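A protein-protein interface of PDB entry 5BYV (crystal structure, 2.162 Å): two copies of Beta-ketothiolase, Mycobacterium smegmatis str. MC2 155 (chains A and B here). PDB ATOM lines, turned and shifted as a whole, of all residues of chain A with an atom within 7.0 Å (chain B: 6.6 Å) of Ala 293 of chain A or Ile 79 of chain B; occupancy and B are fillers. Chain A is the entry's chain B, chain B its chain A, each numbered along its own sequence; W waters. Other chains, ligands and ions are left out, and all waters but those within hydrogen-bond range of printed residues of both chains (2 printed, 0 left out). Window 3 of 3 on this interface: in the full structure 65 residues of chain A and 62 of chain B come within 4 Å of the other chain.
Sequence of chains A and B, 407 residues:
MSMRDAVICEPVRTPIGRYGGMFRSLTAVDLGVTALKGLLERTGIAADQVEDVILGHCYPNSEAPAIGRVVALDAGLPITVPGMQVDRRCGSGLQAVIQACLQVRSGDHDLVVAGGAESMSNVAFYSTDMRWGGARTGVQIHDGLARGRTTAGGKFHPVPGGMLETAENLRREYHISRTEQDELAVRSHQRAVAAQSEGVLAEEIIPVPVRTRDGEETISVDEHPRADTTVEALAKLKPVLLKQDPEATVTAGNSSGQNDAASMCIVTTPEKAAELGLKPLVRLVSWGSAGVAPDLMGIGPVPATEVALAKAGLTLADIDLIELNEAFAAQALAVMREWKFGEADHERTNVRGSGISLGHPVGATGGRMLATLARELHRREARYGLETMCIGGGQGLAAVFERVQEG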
ATOM      1  N   HIS A 157     -21.116 -11.602 -20.943  1.00  0.00           N
ATOM      2  CA  HIS A 157     -21.037 -12.966 -20.410  1.00  0.00           C
ATOM      3  C   HIS A 157     -22.396 -13.645 -20.458  1.00  0.00           C
ATOM      4  O   HIS A 157     -22.996 -13.940 -19.417  1.00  0.00           O
ATOM      5  CB  HIS A 157     -20.484 -12.963 -18.984  1.00  0.00           C
ATOM      6  CG  HIS A 157     -19.286 -12.089 -18.817  1.00  0.00           C
ATOM      7  ND1 HIS A 157     -17.999 -12.568 -18.947  1.00  0.00           N
ATOM      8  CD2 HIS A 157     -19.173 -10.769 -18.544  1.00  0.00           C
ATOM      9  CE1 HIS A 157     -17.146 -11.578 -18.761  1.00  0.00           C
ATOM     10  NE2 HIS A 157     -17.834 -10.475 -18.508  1.00  0.00           N
ATOM     11  N   THR A 166     -24.094 -23.594 -16.254  1.00  0.00           N
ATOM     12  CA  THR A 166     -22.933 -23.335 -15.399  1.00  0.00           C
ATOM     13  C   THR A 166     -22.615 -24.540 -14.546  1.00  0.00           C
ATOM     14  O   THR A 166     -21.473 -24.736 -14.161  1.00  0.00           O
ATOM     15  CB  THR A 166     -23.137 -22.110 -14.456  1.00  0.00           C
ATOM     16  OG1 THR A 166     -24.126 -22.412 -13.463  1.00  0.00           O
ATOM     17  CG2 THR A 166     -23.563 -20.886 -15.225  1.00  0.00           C
ATOM     18  N   ALA A 290     -17.652 -11.990  -3.205  1.00  0.00           N
ATOM     19  CA  ALA A 290     -16.703 -12.129  -4.297  1.00  0.00           C
ATOM     20  C   ALA A 290     -17.406 -12.208  -5.645  1.00  0.00           C
ATOM     21  O   ALA A 290     -18.576 -12.530  -5.723  1.00  0.00           O
ATOM     22  CB  ALA A 290     -15.848 -13.360  -4.084  1.00  0.00           C
ATOM     23  N   GLY A 291     -16.682 -11.896  -6.707  1.00  0.00           N
ATOM     24  CA  GLY A 291     -17.184 -12.118  -8.045  1.00  0.00           C
ATOM     25  C   GLY A 291     -16.364 -13.181  -8.765  1.00  0.00           C
ATOM     26  O   GLY A 291     -15.127 -13.182  -8.685  1.00  0.00           O
ATOM     27  N   VAL A 292     -17.065 -14.081  -9.459  1.00  0.00           N
ATOM     28  CA  VAL A 292     -16.463 -15.101 -10.319  1.00  0.00           C
ATOM     29  C   VAL A 292     -17.081 -15.014 -11.715  1.00  0.00           C
ATOM     30  O   VAL A 292     -18.040 -14.261 -11.919  1.00  0.00           O
ATOM     31  CB  VAL A 292     -16.672 -16.510  -9.750  1.00  0.00           C
ATOM     32  CG1 VAL A 292     -16.039 -16.613  -8.376  1.00  0.00           C
ATOM     33  CG2 VAL A 292     -18.175 -16.845  -9.684  1.00  0.00           C
ATOM     34  N   ALA A 293     -16.545 -15.764 -12.675  1.00  0.00           N
ATOM     35  CA  ALA A 293     -17.123 -15.782 -14.017  1.00  0.00           C
ATOM     36  C   ALA A 293     -18.585 -16.184 -13.954  1.00  0.00           C
ATOM     37  O   ALA A 293     -18.938 -17.136 -13.266  1.00  0.00           O
ATOM     38  CB  ALA A 293     -16.358 -16.734 -14.925  1.00  0.00           C
ATOM     39  N   PRO A 294     -19.451 -15.452 -14.661  1.00  0.00           N
ATOM     40  CA  PRO A 294     -20.869 -15.832 -14.673  1.00  0.00           C
ATOM     41  C   PRO A 294     -21.122 -17.282 -15.122  1.00  0.00           C
ATOM     42  O   PRO A 294     -22.014 -17.944 -14.572  1.00  0.00           O
ATOM     43  CB  PRO A 294     -21.480 -14.832 -15.659  1.00  0.00           C
ATOM     44  CG  PRO A 294     -20.630 -13.628 -15.509  1.00  0.00           C
ATOM     45  CD  PRO A 294     -19.225 -14.143 -15.293  1.00  0.00           C
ATOM     46  N   ASP A 295     -20.348 -17.785 -16.080  1.00  0.00           N
ATOM     47  CA  ASP A 295     -20.574 -19.153 -16.551  1.00  0.00           C
ATOM     48  C   ASP A 295     -19.985 -20.212 -15.616  1.00  0.00           C
ATOM     49  O   ASP A 295     -20.040 -21.404 -15.907  1.00  0.00           O
ATOM     50  CB  ASP A 295     -20.022 -19.336 -17.967  1.00  0.00           C
ATOM     51  CG  ASP A 295     -18.528 -19.174 -18.041  1.00  0.00           C
ATOM     52  OD1 ASP A 295     -17.916 -18.654 -17.090  1.00  0.00           O
ATOM     53  OD2 ASP A 295     -17.954 -19.571 -19.071  1.00  0.00           O
ATOM     54  N   LEU A 296     -19.430 -19.761 -14.495  1.00  0.00           N
ATOM     55  CA  LEU A 296     -18.907 -20.634 -13.459  1.00  0.00           C
ATOM     56  C   LEU A 296     -19.329 -20.136 -12.110  1.00  0.00           C
ATOM     57  O   LEU A 296     -18.667 -20.422 -11.117  1.00  0.00           O
ATOM     58  CB  LEU A 296     -17.385 -20.699 -13.501  1.00  0.00           C
ATOM     59  CG  LEU A 296     -16.764 -21.395 -14.699  1.00  0.00           C
ATOM     60  CD1 LEU A 296     -15.255 -21.244 -14.636  1.00  0.00           C
ATOM     61  CD2 LEU A 296     -17.195 -22.850 -14.685  1.00  0.00           C
ATOM     62  N   MET A 297     -20.389 -19.334 -12.106  1.00  0.00           N
ATOM     63  CA  MET A 297     -21.032 -18.837 -10.896  1.00  0.00           C
ATOM     64  C   MET A 297     -21.028 -19.799  -9.678  1.00  0.00           C
ATOM     65  O   MET A 297     -20.916 -19.337  -8.544  1.00  0.00           O
ATOM     66  CB  MET A 297     -22.464 -18.462 -11.242  1.00  0.00           C
ATOM     67  CG  MET A 297     -23.218 -19.748 -11.489  1.00  0.00           C
ATOM     68  SD  MET A 297     -24.758 -19.903 -10.689  1.00  0.00           S
ATOM     69  CE  MET A 297     -24.094 -19.956  -9.125  1.00  0.00           C
ATOM     70  N   GLY A 298     -21.149 -21.118  -9.894  1.00  0.00           N
ATOM     71  CA  GLY A 298     -21.298 -22.078  -8.804  1.00  0.00           C
ATOM     72  C   GLY A 298     -20.107 -22.188  -7.864  1.00  0.00           C
ATOM     73  O   GLY A 298     -20.203 -22.757  -6.774  1.00  0.00           O
ATOM     74  N   ILE A 299     -18.984 -21.621  -8.282  1.00  0.00           N
ATOM     75  CA  ILE A 299     -17.752 -21.696  -7.513  1.00  0.00           C
ATOM     76  C   ILE A 299     -17.584 -20.472  -6.620  1.00  0.00           C
ATOM     77  O   ILE A 299     -16.644 -20.396  -5.825  1.00  0.00           O
ATOM     78  CB  ILE A 299     -16.516 -21.844  -8.453  1.00  0.00           C
ATOM     79  CG1 ILE A 299     -15.419 -22.689  -7.791  1.00  0.00           C
ATOM     80  CG2 ILE A 299     -16.003 -20.486  -8.932  1.00  0.00           C
ATOM     81  CD1 ILE A 299     -15.846 -24.128  -7.504  1.00  0.00           C
ATOM     82  N   GLY A 300     -18.507 -19.521  -6.754  1.00  0.00           N
ATOM     83  CA  GLY A 300     -18.533 -18.323  -5.920  1.00  0.00           C
ATOM     84  C   GLY A 300     -18.235 -18.466  -4.430  1.00  0.00           C
ATOM     85  O   GLY A 300     -17.546 -17.623  -3.865  1.00  0.00           O
ATOM     86  N   ILE A 391     -23.956 -17.583  -6.326  1.00  0.00           N
ATOM     87  CA  ILE A 391     -24.984 -16.661  -6.769  1.00  0.00           C
ATOM     88  C   ILE A 391     -25.026 -16.554  -8.291  1.00  0.00           C
ATOM     89  O   ILE A 391     -23.963 -16.448  -8.952  1.00  0.00           O
ATOM     90  CB  ILE A 391     -24.745 -15.268  -6.151  1.00  0.00           C
ATOM     91  CG1 ILE A 391     -24.993 -15.293  -4.626  1.00  0.00           C
ATOM     92  CG2 ILE A 391     -25.554 -14.203  -6.852  1.00  0.00           C
ATOM     93  CD1 ILE A 391     -24.412 -14.182  -3.796  1.00  0.00           C
ATOM     94  N   GLY A 393     -25.177 -15.168 -11.852  1.00  0.00           N
ATOM     95  CA  GLY A 393     -24.539 -14.007 -12.426  1.00  0.00           C
ATOM     96  C   GLY A 393     -23.067 -13.990 -12.088  1.00  0.00           C
ATOM     97  O   GLY A 393     -22.322 -13.124 -12.547  1.00  0.00           O
ATOM     98  N   GLY A 394     -22.643 -14.947 -11.267  1.00  0.00           N
ATOM     99  CA  GLY A 394     -21.240 -15.054 -10.906  1.00  0.00           C
ATOM    100  C   GLY A 394     -20.822 -14.265  -9.676  1.00  0.00           C
ATOM    101  O   GLY A 394     -19.978 -13.372  -9.740  1.00  0.00           O
ATOM    102  N   GLN A 395     -21.419 -14.602  -8.540  1.00  0.00           N
ATOM    103  CA  GLN A 395     -21.001 -14.041  -7.262  1.00  0.00           C
ATOM    104  C   GLN A 395     -21.014 -15.129  -6.211  1.00  0.00           C
ATOM    105  O   GLN A 395     -21.648 -16.179  -6.394  1.00  0.00           O
ATOM    106  CB  GLN A 395     -21.923 -12.897  -6.832  1.00  0.00           C
ATOM    107  CG  GLN A 395     -21.950 -11.718  -7.754  1.00  0.00           C
ATOM    108  CD  GLN A 395     -22.784 -10.597  -7.202  1.00  0.00           C
ATOM    109  OE1 GLN A 395     -22.343  -9.883  -6.319  1.00  0.00           O
ATOM    110  NE2 GLN A 395     -23.992 -10.426  -7.730  1.00  0.00           N
ATOM    111  N   ARG B  69     -24.555  -5.606 -10.353  1.00  0.00           N
ATOM    112  CA  ARG B  69     -23.612  -6.538 -10.966  1.00  0.00           C
ATOM    113  C   ARG B  69     -23.650  -6.450 -12.483  1.00  0.00           C
ATOM    114  O   ARG B  69     -22.610  -6.480 -13.141  1.00  0.00           O
ATOM    115  CB  ARG B  69     -23.912  -7.974 -10.506  1.00  0.00           C
ATOM    116  CG  ARG B  69     -23.188  -9.101 -11.277  1.00  0.00           C
ATOM    117  CD  ARG B  69     -21.728  -9.341 -10.872  1.00  0.00           C
ATOM    118  NE  ARG B  69     -21.211 -10.539 -11.543  1.00  0.00           N
ATOM    119  CZ  ARG B  69     -19.933 -10.915 -11.582  1.00  0.00           C
ATOM    120  NH1 ARG B  69     -18.992 -10.199 -10.990  1.00  0.00           N
ATOM    121  NH2 ARG B  69     -19.595 -12.014 -12.230  1.00  0.00           N
ATOM    122  N   LEU B  73     -20.568  -5.321 -14.905  1.00  0.00           N
ATOM    123  CA  LEU B  73     -20.021  -6.125 -15.994  1.00  0.00           C
ATOM    124  C   LEU B  73     -20.178  -5.463 -17.363  1.00  0.00           C
ATOM    125  O   LEU B  73     -19.228  -5.436 -18.141  1.00  0.00           O
ATOM    126  CB  LEU B  73     -20.656  -7.511 -16.009  1.00  0.00           C
ATOM    127  CG  LEU B  73     -20.336  -8.372 -14.785  1.00  0.00           C
ATOM    128  CD1 LEU B  73     -21.124  -9.691 -14.806  1.00  0.00           C
ATOM    129  CD2 LEU B  73     -18.825  -8.612 -14.693  1.00  0.00           C
ATOM    130  N   LEU B  77     -16.130  -3.606 -15.949  1.00  0.00           N
ATOM    131  CA  LEU B  77     -15.397  -3.947 -14.730  1.00  0.00           C
ATOM    132  C   LEU B  77     -15.157  -5.444 -14.777  1.00  0.00           C
ATOM    133  O   LEU B  77     -15.914  -6.155 -15.437  1.00  0.00           O
ATOM    134  CB  LEU B  77     -16.180  -3.526 -13.472  1.00  0.00           C
ATOM    135  CG  LEU B  77     -16.112  -2.051 -13.024  1.00  0.00           C
ATOM    136  CD1 LEU B  77     -16.604  -1.100 -14.093  1.00  0.00           C
ATOM    137  CD2 LEU B  77     -16.884  -1.790 -11.730  1.00  0.00           C
ATOM    138  N   PRO B  78     -14.094  -5.939 -14.115  1.00  0.00           N
ATOM    139  CA  PRO B  78     -13.818  -7.380 -14.192  1.00  0.00           C
ATOM    140  C   PRO B  78     -14.864  -8.236 -13.467  1.00  0.00           C
ATOM    141  O   PRO B  78     -15.632  -7.733 -12.645  1.00  0.00           O
ATOM    142  CB  PRO B  78     -12.441  -7.513 -13.528  1.00  0.00           C
ATOM    143  CG  PRO B  78     -12.319  -6.316 -12.640  1.00  0.00           C
ATOM    144  CD  PRO B  78     -13.064  -5.215 -13.345  1.00  0.00           C
ATOM    145  N   ILE B  79     -14.870  -9.532 -13.763  1.00  0.00           N
ATOM    146  CA  ILE B  79     -15.843 -10.457 -13.196  1.00  0.00           C
ATOM    147  C   ILE B  79     -15.711 -10.569 -11.689  1.00  0.00           C
ATOM    148  O   ILE B  79     -16.565 -11.158 -11.039  1.00  0.00           O
ATOM    149  CB  ILE B  79     -15.704 -11.856 -13.813  1.00  0.00           C
ATOM    150  CG1 ILE B  79     -14.254 -12.323 -13.722  1.00  0.00           C
ATOM    151  CG2 ILE B  79     -16.198 -11.865 -15.254  1.00  0.00           C
ATOM    152  CD1 ILE B  79     -14.081 -13.773 -14.075  1.00  0.00           C
ATOM    153  N   THR B  80     -14.644  -9.994 -11.141  1.00  0.00           N
ATOM    154  CA  THR B  80     -14.382 -10.045  -9.708  1.00  0.00           C
ATOM    155  C   THR B  80     -15.166  -8.996  -8.897  1.00  0.00           C
ATOM    156  O   THR B  80     -15.125  -8.997  -7.670  1.00  0.00           O
ATOM    157  CB  THR B  80     -12.872  -9.879  -9.431  1.00  0.00           C
ATOM    158  OG1 THR B  80     -12.375  -8.709 -10.094  1.00  0.00           O
ATOM    159  CG2 THR B  80     -12.132 -11.071  -9.937  1.00  0.00           C
ATOM    160  N   VAL B  81     -15.885  -8.115  -9.581  1.00  0.00           N
ATOM    161  CA  VAL B  81     -16.633  -7.060  -8.907  1.00  0.00           C
ATOM    162  C   VAL B  81     -18.089  -7.456  -8.598  1.00  0.00           C
ATOM    163  O   VAL B  81     -18.915  -7.560  -9.509  1.00  0.00           O
ATOM    164  CB  VAL B  81     -16.640  -5.781  -9.739  1.00  0.00           C
ATOM    165  CG1 VAL B  81     -17.425  -4.690  -9.015  1.00  0.00           C
ATOM    166  CG2 VAL B  81     -15.206  -5.334 -10.026  1.00  0.00           C
ATOM    167  N   PRO B  82     -18.406  -7.666  -7.302  1.00  0.00           N
ATOM    168  CA  PRO B  82     -19.773  -8.018  -6.884  1.00  0.00           C
ATOM    169  C   PRO B  82     -20.759  -6.858  -7.094  1.00  0.00           C
ATOM    170  O   PRO B  82     -20.336  -5.715  -7.255  1.00  0.00           O
ATOM    171  CB  PRO B  82     -19.611  -8.352  -5.394  1.00  0.00           C
ATOM    172  CG  PRO B  82     -18.127  -8.537  -5.181  1.00  0.00           C
ATOM    173  CD  PRO B  82     -17.492  -7.592  -6.150  1.00  0.00           C
HETATM  174  O   HOH W   1     -14.064 -10.812  -5.958  1.00  0.00           O
HETATM  175  O   HOH W   2     -16.698  -7.367 -18.241  1.00  0.00           O
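The guanidinium group of Arg 69 of chain B lies within hydrogen-bond range of the backbone carbonyl oxygen of Val 292 of chain A, at 2.8 Å.
O of Gly 393 of chain A sits at hydrogen-bond distance from NH2 of Arg 69 of chain B (3.0 Å).
O of Gly 394 of chain A lies within hydrogen-bond range of NH2 of Arg 69 of chain B (2.9 Å).
The backbone NH (N) of Val 292 of chain A lies within hydrogen-bond range of the backbone carbonyl oxygen (O) of Ile 79 of chain B, 3.4 Å away.
The backbone NH (N) of Gly 291 of chain A is in hydrogen-bond range of the backbone carbonyl oxygen (O) of Thr 80 of chain B.
The backbone carbonyl oxygen of Gly 291 of chain A lies close to the backbone carbonyl oxygen of Ile 79 of chain B (3.4 Å).
The guanidinium group of Arg 69 of chain B lies within hydrogen-bond range of the backbone carbonyl oxygen of Ile 79 of chain B (2.6 Å).
NH1 of Arg 69 of chain B lies within hydrogen-bond range of O of Val 81 of chain B (3.0 Å).
The backbone NH of Val 292 of chain A lies within hydrogen-bond range of the backbone carbonyl oxygen of Gly 394 of chain A (3.0 Å).
Among the printed residues, pairs that only touch across the chains: His 157 of chain A with Ile 79 of chain B (3.6 Å), Ala 290 of chain A with Pro 82 of chain B (3.8 Å), Gly 291 of chain A with Arg 69 of chain B (3.95 Å), Gly 291 of chain A with Pro 82 of chain B (3.96 Å), Ala 293 of chain A with Ile 79 of chain B (3.5 Å), Pro 294 of chain A with Arg 69 of chain B (3.7 Å), Pro 294 of chain A with Ile 79 of chain B (3.8 Å), Gln 395 of chain A with Arg 69 of chain B (3.7 Å) and Gln 395 of chain A with Pro 82 of chain B (3.2 Å).
Of chain B, only Ile 79 (3.5 Å) comes within 4 Å of Ala 293 of chain A.
Of chain A, only His 157 (3.6 Å), Gly 291 (3.1 Å), Val 292 (3.4 Å), Ala 293 (3.5 Å) and Pro 294 (3.8 Å) come within 4 Å of Ile 79 of chain B.
Of the printed residues of chain B, Gly 393 of chain A touches Arg 69.
Of the printed residues of chain A, Arg 69 of chain B touches Gly 291, Val 292, Pro 294, Gly 393, Gly 394 and Gln 395.
Of the printed residues of chain B, Ala 290 of chain A touches Pro 82 (3.8 Å).
Printed residues of chain B within 4 Å of Pro 294 of chain A: Arg 69 (3.7 Å) and Ile 79 (3.8 Å).
Gly 298 of chain A touches none of the printed residues of chain B.
The nearest residue of chain A that does not touch Ile 79 of chain B is Gly 394 of chain A (4.3 Å).
Of the 17 printed residues of chain A, 9 touch a printed residue of chain B.
Printed residues of chain A that touch a printed residue of chain B: His 157, Ala 290, Gly 291, Val 292, Ala 293, Pro 294, Gly 393, Gly 394 and Gln 395.
Hydrophobic or aromatic side chains of chain A within 4 Å of the printed part of chain B: His 157, Ala 293 and Pro 294.
Printed residues of chain B that touch a printed residue of chain A: Arg 69, Ile 79, Thr 80 and Pro 82.
Hydrophobic or aromatic side chains of chain B within 4 Å of the printed part of chain A: Ile 79 and Pro 82.
No position is printed for both chains.
Of the 15 pairs that touch across the chains among the printed residues, none has its exchanged pair printed and touching as well.
Water W1 lies within hydrogen-bond range of the backbone carbonyl oxygen (O) of Thr 80 of chain B and the backbone NH (N) of Gly 291 of chain A.
Water W2 lies within hydrogen-bond range of the backbone carbonyl oxygen of Leu 77 of chain B (3.2 Å), the backbone carbonyl oxygen of Leu 73 of chain B (3.2 Å) and a ring nitrogen (NE2) of His 157 of chain A (3.3 Å).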
